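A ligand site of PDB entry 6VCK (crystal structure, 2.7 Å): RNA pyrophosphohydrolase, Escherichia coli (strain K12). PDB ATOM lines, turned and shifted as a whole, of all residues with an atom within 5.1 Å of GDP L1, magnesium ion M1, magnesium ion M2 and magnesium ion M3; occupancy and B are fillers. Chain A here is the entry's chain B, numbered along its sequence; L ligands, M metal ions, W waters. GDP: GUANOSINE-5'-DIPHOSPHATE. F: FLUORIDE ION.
Magnesium ion M1 is bound by water W2 (2.1 Å), F of F L2 (2.2 Å), O3B of GDP L1 (2.3 Å) and OE2 of Glu 54 (2.4 Å). Magnesium ion M1 has four donor atoms within binding distance.
Magnesium ion M3 is bound by O of Gln 38. Slightly farther from magnesium ion M3 lies O1A of GDP L1 (2.7 Å). Slightly farther from magnesium ion M3 lies the side-chain carboxylate (OE1) of Glu 121 (2.7 Å). Slightly farther from magnesium ion M3 lies the side-chain carboxylate (OE2) of Glu 121 (2.8 Å).
Gln 35 touches GDP L1 (OE1 to O6, 3.9 Å). CA of Gly 39 touches O3A of GDP L1, 3.1 Å away. Tyr 78 touches GDP L1 (OH to C8, 3.7 Å). Leu 80 touches GDP L1 (CD2 to O2', 3.97 Å). CZ of Phe 140 touches C6 of GDP L1, at 3.9 Å. Within 4 Å of GDP L1: Asn 11, Arg 28, Gln 35, Gln 38, Gly 39, Gly 40, Glu 54, Tyr 78, Leu 80, Gln 96, Glu 121, Phe 140 and Lys 141.
Magnesium ion M2 is bound by an oxygen (O2B) of GDP L1 (2.0 Å), a fluorine (F) of F L2 (2.2 Å), the side-chain carboxylate (OE1) of Glu 121 (2.3 Å) and the side-chain carboxylate (OE1) of Glu 54 (2.4 Å). Magnesium ion M2 has four donor atoms within binding distance.
Two residues have an atom within 4 Å of magnesium ion M3: Gln 38 and Glu 121.
Water W2 bridges the backbone carbonyl oxygen of Gly 40 (2.8 Å) and the side-chain amide oxygen of Asn 42 (3.2 Å). Water W1 bridges O6 of GDP L1 and OE1 of Gln 35.
The backbone NH of Gly 40 sits close to the side-chain carboxylate of Glu 54 (3.4 Å). The side-chain amino group of Lys 141 is in hydrogen-bond range of the side-chain amide oxygen of Gln 35, 3.3 Å away. N of Gln 96 is in hydrogen-bond range of O of Tyr 78. The guanidinium group of Arg 53 lies within salt-bridge range of the side-chain carboxylate of Glu 57 (3.0 Å). The side-chain amide oxygen (OE1) of Gln 35 sits at hydrogen-bond distance from the guanidinium group (NH2) of Arg 28 (2.6 Å). The guanidinium group (NH1) of Arg 53 is in hydrogen-bond range of the backbone carbonyl oxygen (O) of Gly 40, at 3.1 Å. The guanidinium group (NH1) of Arg 53 lies close to the side-chain amide nitrogen (ND2) of Asn 42 (3.3 Å). NE2 of Gln 38 lies within hydrogen-bond range of OH of Tyr 78, at 2.9 Å.
Merely in contact with magnesium ion M1: Arg 53 (3.9 Å). Within 4 Å of magnesium ion M1: Arg 53 and Glu 54. Along chain A the residues within 4 Å of magnesium ion M1 span positions 53 to 54. The nearest printed residue that does not touch magnesium ion M1 is Gly 40 (4.1 Å).
Residues that only touch magnesium ion M2: Glu 58 (3.7 Å). Of the 21 residues printed, 3 come within 4 Å of magnesium ion M2.
N3 of GDP L1 lies close to NH1 of Arg 28, 3.2 Å away. The side-chain amino group (NZ) of Lys 141 lies within hydrogen-bond range of a nitrogen (N7) of GDP L1, 3.1 Å away. The backbone carbonyl oxygen (O) of Gln 38 lies close to an oxygen (O1A) of GDP L1, at 2.8 Å. The side-chain amide nitrogen (ND2) of Asn 11 is in hydrogen-bond range of an oxygen (O2A) of GDP L1 (2.9 Å). N of Gly 40 lies within hydrogen-bond range of O3A of GDP L1 (3.2 Å). The side-chain amide nitrogen (NE2) of Gln 96 lies within hydrogen-bond range of an oxygen (O4') of GDP L1 (2.9 Å). An oxygen (O2A) of GDP L1 lies within hydrogen-bond range of the side-chain amide nitrogen (NE2) of Gln 38 (3.4 Å).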
ATOM      1  N   ASN A  11     -29.197  16.295   7.974  1.00  0.00           N
ATOM      2  CA  ASN A  11     -28.437  15.050   8.025  1.00  0.00           C
ATOM      3  C   ASN A  11     -28.067  14.634   6.606  1.00  0.00           C
ATOM      4  O   ASN A  11     -28.612  15.143   5.629  1.00  0.00           O
ATOM      5  CB  ASN A  11     -29.225  13.945   8.741  1.00  0.00           C
ATOM      6  CG  ASN A  11     -28.346  12.830   9.240  1.00  0.00           C
ATOM      7  OD1 ASN A  11     -27.816  12.041   8.458  1.00  0.00           O
ATOM      8  ND2 ASN A  11     -28.188  12.744  10.558  1.00  0.00           N
ATOM      9  N   ARG A  28     -23.748  -0.647  14.536  1.00  0.00           N
ATOM     10  CA  ARG A  28     -23.516   0.424  15.491  1.00  0.00           C
ATOM     11  C   ARG A  28     -22.582  -0.034  16.611  1.00  0.00           C
ATOM     12  O   ARG A  28     -22.588  -1.191  17.007  1.00  0.00           O
ATOM     13  CB  ARG A  28     -24.834   0.923  16.084  1.00  0.00           C
ATOM     14  CG  ARG A  28     -25.561   1.939  15.225  1.00  0.00           C
ATOM     15  CD  ARG A  28     -25.267   3.347  15.691  1.00  0.00           C
ATOM     16  NE  ARG A  28     -26.215   3.783  16.705  1.00  0.00           N
ATOM     17  CZ  ARG A  28     -27.368   4.392  16.429  1.00  0.00           C
ATOM     18  NH1 ARG A  28     -28.170   4.766  17.419  1.00  0.00           N
ATOM     19  NH2 ARG A  28     -27.710   4.642  15.171  1.00  0.00           N
ATOM     20  N   GLN A  35     -27.157  -0.476  10.027  1.00  0.00           N
ATOM     21  CA  GLN A  35     -27.713   0.639   9.281  1.00  0.00           C
ATOM     22  C   GLN A  35     -26.682   1.136   8.281  1.00  0.00           C
ATOM     23  O   GLN A  35     -25.528   0.704   8.265  1.00  0.00           O
ATOM     24  CB  GLN A  35     -28.129   1.778  10.210  1.00  0.00           C
ATOM     25  CG  GLN A  35     -26.973   2.401  10.965  1.00  0.00           C
ATOM     26  CD  GLN A  35     -27.403   3.573  11.825  1.00  0.00           C
ATOM     27  OE1 GLN A  35     -27.988   3.384  12.894  1.00  0.00           O
ATOM     28  NE2 GLN A  35     -27.112   4.782  11.367  1.00  0.00           N
ATOM     29  N   PRO A  37     -24.375   4.325   6.904  1.00  0.00           N
ATOM     30  CA  PRO A  37     -23.716   5.462   7.554  1.00  0.00           C
ATOM     31  C   PRO A  37     -24.481   6.754   7.287  1.00  0.00           C
ATOM     32  O   PRO A  37     -24.782   7.085   6.139  1.00  0.00           O
ATOM     33  CB  PRO A  37     -22.326   5.497   6.912  1.00  0.00           C
ATOM     34  CG  PRO A  37     -22.148   4.152   6.264  1.00  0.00           C
ATOM     35  CD  PRO A  37     -23.522   3.694   5.886  1.00  0.00           C
ATOM     36  N   GLN A  38     -24.828   7.458   8.365  1.00  0.00           N
ATOM     37  CA  GLN A  38     -25.415   8.780   8.245  1.00  0.00           C
ATOM     38  C   GLN A  38     -24.780   9.688   9.292  1.00  0.00           C
ATOM     39  O   GLN A  38     -24.290   9.232  10.320  1.00  0.00           O
ATOM     40  CB  GLN A  38     -26.940   8.748   8.398  1.00  0.00           C
ATOM     41  CG  GLN A  38     -27.444   8.445   9.791  1.00  0.00           C
ATOM     42  CD  GLN A  38     -28.915   8.085   9.789  1.00  0.00           C
ATOM     43  OE1 GLN A  38     -29.368   7.254   8.995  1.00  0.00           O
ATOM     44  NE2 GLN A  38     -29.681   8.715  10.684  1.00  0.00           N
ATOM     45  N   GLY A  39     -24.807  10.985   9.006  1.00  0.00           N
ATOM     46  CA  GLY A  39     -24.153  11.948   9.870  1.00  0.00           C
ATOM     47  C   GLY A  39     -24.797  13.316   9.789  1.00  0.00           C
ATOM     48  O   GLY A  39     -25.438  13.664   8.794  1.00  0.00           O
ATOM     49  N   GLY A  40     -24.607  14.089  10.857  1.00  0.00           N
ATOM     50  CA  GLY A  40     -25.226  15.406  10.932  1.00  0.00           C
ATOM     51  C   GLY A  40     -24.434  16.460  10.173  1.00  0.00           C
ATOM     52  O   GLY A  40     -23.207  16.473  10.190  1.00  0.00           O
ATOM     53  N   ASN A  42     -22.863  20.030   9.668  1.00  0.00           N
ATOM     54  CA  ASN A  42     -22.222  20.952  10.585  1.00  0.00           C
ATOM     55  C   ASN A  42     -22.410  22.394  10.105  1.00  0.00           C
ATOM     56  O   ASN A  42     -22.695  22.632   8.930  1.00  0.00           O
ATOM     57  CB  ASN A  42     -20.722  20.630  10.723  1.00  0.00           C
ATOM     58  CG  ASN A  42     -20.471  19.514  11.713  1.00  0.00           C
ATOM     59  OD1 ASN A  42     -21.323  19.180  12.528  1.00  0.00           O
ATOM     60  ND2 ASN A  42     -19.272  18.930  11.643  1.00  0.00           N
ATOM     61  N   ARG A  53     -16.946  14.214   4.849  1.00  0.00           N
ATOM     62  CA  ARG A  53     -16.379  14.195   6.195  1.00  0.00           C
ATOM     63  C   ARG A  53     -16.858  12.963   6.952  1.00  0.00           C
ATOM     64  O   ARG A  53     -16.046  12.183   7.467  1.00  0.00           O
ATOM     65  CB  ARG A  53     -16.768  15.474   6.945  1.00  0.00           C
ATOM     66  CG  ARG A  53     -16.101  15.608   8.304  1.00  0.00           C
ATOM     67  CD  ARG A  53     -16.572  16.873   9.009  1.00  0.00           C
ATOM     68  NE  ARG A  53     -18.011  17.052   8.885  1.00  0.00           N
ATOM     69  CZ  ARG A  53     -18.921  16.411   9.610  1.00  0.00           C
ATOM     70  NH1 ARG A  53     -20.215  16.646   9.418  1.00  0.00           N
ATOM     71  NH2 ARG A  53     -18.535  15.543  10.537  1.00  0.00           N
ATOM     72  N   GLU A  54     -18.180  12.757   7.013  1.00  0.00           N
ATOM     73  CA  GLU A  54     -18.728  11.594   7.710  1.00  0.00           C
ATOM     74  C   GLU A  54     -18.255  10.290   7.073  1.00  0.00           C
ATOM     75  O   GLU A  54     -18.067   9.290   7.778  1.00  0.00           O
ATOM     76  CB  GLU A  54     -20.257  11.655   7.728  1.00  0.00           C
ATOM     77  CG  GLU A  54     -20.820  12.841   8.506  1.00  0.00           C
ATOM     78  CD  GLU A  54     -20.870  12.600  10.007  1.00  0.00           C
ATOM     79  OE1 GLU A  54     -20.561  11.470  10.437  1.00  0.00           O
ATOM     80  OE2 GLU A  54     -21.207  13.536  10.757  1.00  0.00           O
ATOM     81  N   GLU A  57     -14.854   9.886   8.489  1.00  0.00           N
ATOM     82  CA  GLU A  57     -14.899   9.798   9.942  1.00  0.00           C
ATOM     83  C   GLU A  57     -15.341   8.416  10.407  1.00  0.00           C
ATOM     84  O   GLU A  57     -14.788   7.870  11.364  1.00  0.00           O
ATOM     85  CB  GLU A  57     -15.833  10.865  10.508  1.00  0.00           C
ATOM     86  CG  GLU A  57     -15.240  12.266  10.557  1.00  0.00           C
ATOM     87  CD  GLU A  57     -16.204  13.265  11.180  1.00  0.00           C
ATOM     88  OE1 GLU A  57     -17.382  12.914  11.397  1.00  0.00           O
ATOM     89  OE2 GLU A  57     -15.770  14.412  11.452  1.00  0.00           O
ATOM     90  N   GLU A  58     -16.344   7.842   9.739  1.00  0.00           N
ATOM     91  CA  GLU A  58     -16.904   6.584  10.203  1.00  0.00           C
ATOM     92  C   GLU A  58     -16.550   5.387   9.347  1.00  0.00           C
ATOM     93  O   GLU A  58     -16.453   4.283   9.879  1.00  0.00           O
ATOM     94  CB  GLU A  58     -18.435   6.692  10.317  1.00  0.00           C
ATOM     95  CG  GLU A  58     -18.882   7.484  11.541  1.00  0.00           C
ATOM     96  CD  GLU A  58     -18.010   7.209  12.757  1.00  0.00           C
ATOM     97  OE1 GLU A  58     -17.401   8.165  13.294  1.00  0.00           O
ATOM     98  OE2 GLU A  58     -17.934   6.037  13.200  1.00  0.00           O
ATOM     99  N   TYR A  78     -37.739  11.742   8.919  1.00  0.00           N
ATOM    100  CA  TYR A  78     -38.268  10.686   9.774  1.00  0.00           C
ATOM    101  C   TYR A  78     -38.265  11.177  11.213  1.00  0.00           C
ATOM    102  O   TYR A  78     -37.280  11.784  11.650  1.00  0.00           O
ATOM    103  CB  TYR A  78     -37.473   9.387   9.616  1.00  0.00           C
ATOM    104  CG  TYR A  78     -36.085   9.360  10.235  1.00  0.00           C
ATOM    105  CD1 TYR A  78     -35.896   9.034  11.584  1.00  0.00           C
ATOM    106  CD2 TYR A  78     -34.956   9.610   9.464  1.00  0.00           C
ATOM    107  CE1 TYR A  78     -34.632   9.001  12.142  1.00  0.00           C
ATOM    108  CE2 TYR A  78     -33.694   9.569  10.010  1.00  0.00           C
ATOM    109  CZ  TYR A  78     -33.529   9.271  11.353  1.00  0.00           C
ATOM    110  OH  TYR A  78     -32.258   9.236  11.877  1.00  0.00           O
ATOM    111  N   LEU A  80     -38.199  10.724  15.264  1.00  0.00           N
ATOM    112  CA  LEU A  80     -37.664   9.796  16.232  1.00  0.00           C
ATOM    113  C   LEU A  80     -38.799   9.188  17.056  1.00  0.00           C
ATOM    114  O   LEU A  80     -39.875   9.785  17.174  1.00  0.00           O
ATOM    115  CB  LEU A  80     -36.654  10.502  17.136  1.00  0.00           C
ATOM    116  CG  LEU A  80     -35.215  10.584  16.626  1.00  0.00           C
ATOM    117  CD1 LEU A  80     -35.025  11.791  15.729  1.00  0.00           C
ATOM    118  CD2 LEU A  80     -34.236  10.622  17.777  1.00  0.00           C
ATOM    119  N   LEU A  84     -37.465   8.354  22.736  1.00  0.00           N
ATOM    120  CA  LEU A  84     -36.048   8.729  22.720  1.00  0.00           C
ATOM    121  C   LEU A  84     -35.823  10.096  22.087  1.00  0.00           C
ATOM    122  O   LEU A  84     -34.837  10.317  21.382  1.00  0.00           O
ATOM    123  CB  LEU A  84     -35.187   7.667  22.044  1.00  0.00           C
ATOM    124  CG  LEU A  84     -35.101   6.409  22.931  1.00  0.00           C
ATOM    125  CD1 LEU A  84     -35.519   5.114  22.209  1.00  0.00           C
ATOM    126  CD2 LEU A  84     -33.760   6.240  23.665  1.00  0.00           C
ATOM    127  N   GLN A  96     -35.114  13.920  11.928  1.00  0.00           N
ATOM    128  CA  GLN A  96     -33.960  14.244  11.105  1.00  0.00           C
ATOM    129  C   GLN A  96     -34.404  14.439   9.668  1.00  0.00           C
ATOM    130  O   GLN A  96     -35.262  13.713   9.169  1.00  0.00           O
ATOM    131  CB  GLN A  96     -32.893  13.147  11.182  1.00  0.00           C
ATOM    132  CG  GLN A  96     -32.303  12.938  12.578  1.00  0.00           C
ATOM    133  CD  GLN A  96     -30.813  12.673  12.546  1.00  0.00           C
ATOM    134  OE1 GLN A  96     -30.073  13.325  11.815  1.00  0.00           O
ATOM    135  NE2 GLN A  96     -30.375  11.697  13.331  1.00  0.00           N
ATOM    136  N   GLU A 121     -18.518   5.250  15.553  1.00  0.00           N
ATOM    137  CA  GLU A 121     -19.936   4.932  15.583  1.00  0.00           C
ATOM    138  C   GLU A 121     -20.226   3.517  15.113  1.00  0.00           C
ATOM    139  O   GLU A 121     -21.302   2.989  15.402  1.00  0.00           O
ATOM    140  CB  GLU A 121     -20.719   5.921  14.708  1.00  0.00           C
ATOM    141  CG  GLU A 121     -21.380   7.038  15.470  1.00  0.00           C
ATOM    142  CD  GLU A 121     -22.212   7.920  14.561  1.00  0.00           C
ATOM    143  OE1 GLU A 121     -21.635   8.853  13.964  1.00  0.00           O
ATOM    144  OE2 GLU A 121     -23.441   7.690  14.454  1.00  0.00           O
ATOM    145  N   PHE A 122     -19.290   2.890  14.400  1.00  0.00           N
ATOM    146  CA  PHE A 122     -19.474   1.554  13.871  1.00  0.00           C
ATOM    147  C   PHE A 122     -18.264   0.690  14.208  1.00  0.00           C
ATOM    148  O   PHE A 122     -17.116   1.157  14.167  1.00  0.00           O
ATOM    149  CB  PHE A 122     -19.663   1.574  12.337  1.00  0.00           C
ATOM    150  CG  PHE A 122     -20.838   2.395  11.886  1.00  0.00           C
ATOM    151  CD1 PHE A 122     -22.114   2.129  12.345  1.00  0.00           C
ATOM    152  CD2 PHE A 122     -20.656   3.431  10.973  1.00  0.00           C
ATOM    153  CE1 PHE A 122     -23.189   2.884  11.912  1.00  0.00           C
ATOM    154  CE2 PHE A 122     -21.731   4.187  10.540  1.00  0.00           C
ATOM    155  CZ  PHE A 122     -22.999   3.914  11.018  1.00  0.00           C
ATOM    156  N   VAL A 138     -34.109  -0.370  11.358  1.00  0.00           N
ATOM    157  CA  VAL A 138     -35.023  -0.094  12.453  1.00  0.00           C
ATOM    158  C   VAL A 138     -36.275   0.576  11.900  1.00  0.00           C
ATOM    159  O   VAL A 138     -36.237   1.308  10.907  1.00  0.00           O
ATOM    160  CB  VAL A 138     -34.333   0.763  13.531  1.00  0.00           C
ATOM    161  CG1 VAL A 138     -34.130   2.194  13.056  1.00  0.00           C
ATOM    162  CG2 VAL A 138     -35.107   0.719  14.843  1.00  0.00           C
ATOM    163  N   PHE A 140     -38.478   2.942  12.478  1.00  0.00           N
ATOM    164  CA  PHE A 140     -38.760   4.347  12.222  1.00  0.00           C
ATOM    165  C   PHE A 140     -37.916   4.937  11.109  1.00  0.00           C
ATOM    166  O   PHE A 140     -38.100   6.109  10.767  1.00  0.00           O
ATOM    167  CB  PHE A 140     -38.619   5.182  13.512  1.00  0.00           C
ATOM    168  CG  PHE A 140     -37.258   5.093  14.159  1.00  0.00           C
ATOM    169  CD1 PHE A 140     -36.258   5.996  13.811  1.00  0.00           C
ATOM    170  CD2 PHE A 140     -37.003   4.152  15.128  1.00  0.00           C
ATOM    171  CE1 PHE A 140     -35.013   5.923  14.414  1.00  0.00           C
ATOM    172  CE2 PHE A 140     -35.758   4.079  15.732  1.00  0.00           C
ATOM    173  CZ  PHE A 140     -34.760   4.975  15.372  1.00  0.00           C
ATOM    174  N   LYS A 141     -36.990   4.167  10.531  1.00  0.00           N
ATOM    175  CA  LYS A 141     -36.243   4.586   9.348  1.00  0.00           C
ATOM    176  C   LYS A 141     -36.702   3.890   8.079  1.00  0.00           C
ATOM    177  O   LYS A 141     -36.156   4.164   7.003  1.00  0.00           O
ATOM    178  CB  LYS A 141     -34.743   4.331   9.553  1.00  0.00           C
ATOM    179  CG  LYS A 141     -34.022   5.328  10.435  1.00  0.00           C
ATOM    180  CD  LYS A 141     -32.571   4.897  10.634  1.00  0.00           C
ATOM    181  CE  LYS A 141     -31.802   5.876  11.486  1.00  0.00           C
ATOM    182  NZ  LYS A 141     -30.429   5.367  11.772  1.00  0.00           N
HETATM  183  PB  GDP L   1     -23.683  12.004  13.412  1.00  0.00           P
HETATM  184  O1B GDP L   1     -23.690  11.782  14.886  1.00  0.00           O
HETATM  185  O2B GDP L   1     -22.635  11.137  12.777  1.00  0.00           O
HETATM  186  O3B GDP L   1     -23.380  13.448  13.116  1.00  0.00           O
HETATM  187  O3A GDP L   1     -25.108  11.622  12.806  1.00  0.00           O
HETATM  188  PA  GDP L   1     -26.193  10.411  13.171  1.00  0.00           P
HETATM  189  O1A GDP L   1     -25.586   9.031  12.807  1.00  0.00           O
HETATM  190  O2A GDP L   1     -27.488  10.619  12.378  1.00  0.00           O
HETATM  191  O5' GDP L   1     -26.482  10.481  14.808  1.00  0.00           O
HETATM  192  C5' GDP L   1     -27.250   9.505  15.420  1.00  0.00           C
HETATM  193  C4' GDP L   1     -28.274  10.212  16.281  1.00  0.00           C
HETATM  194  O4' GDP L   1     -29.591  10.124  15.665  1.00  0.00           O
HETATM  195  C3' GDP L   1     -28.400   9.521  17.643  1.00  0.00           C
HETATM  196  O3' GDP L   1     -27.696  10.261  18.641  1.00  0.00           O
HETATM  197  C2' GDP L   1     -29.947   9.580  17.910  1.00  0.00           C
HETATM  198  O2' GDP L   1     -30.323  10.853  18.415  1.00  0.00           O
HETATM  199  C1' GDP L   1     -30.471   9.396  16.501  1.00  0.00           C
HETATM  200  N9  GDP L   1     -30.464   7.948  16.123  1.00  0.00           N
HETATM  201  C8  GDP L   1     -30.589   7.827  14.805  1.00  0.00           C
HETATM  202  N7  GDP L   1     -30.706   6.490  14.597  1.00  0.00           N
HETATM  203  C5  GDP L   1     -30.831   5.868  15.778  1.00  0.00           C
HETATM  204  C6  GDP L   1     -31.006   4.530  16.130  1.00  0.00           C
HETATM  205  O6  GDP L   1     -31.076   3.676  15.239  1.00  0.00           O
HETATM  206  N1  GDP L   1     -31.099   4.145  17.400  1.00  0.00           N
HETATM  207  C2  GDP L   1     -31.014   5.140  18.316  1.00  0.00           C
HETATM  208  N2  GDP L   1     -31.104   4.791  19.597  1.00  0.00           N
HETATM  209  N3  GDP L   1     -30.841   6.477  18.076  1.00  0.00           N
HETATM  210  C4  GDP L   1     -30.801   6.847  16.772  1.00  0.00           C
HETATM  211  F     F L   2     -20.484  12.362  13.565  1.00  0.00           F
HETATM  212 MG    MG M   1     -21.210  14.336  13.058  1.00  0.00          MG
HETATM  213 MG    MG M   2     -20.747  10.468  12.558  1.00  0.00          MG
HETATM  214 MG    MG M   3     -23.161   8.506  11.742  1.00  0.00          MG
HETATM  215  O   HOH W   1     -30.647   2.099  13.403  1.00  0.00           O
HETATM  216  O   HOH W   2     -22.253  16.089  12.768  1.00  0.00           O
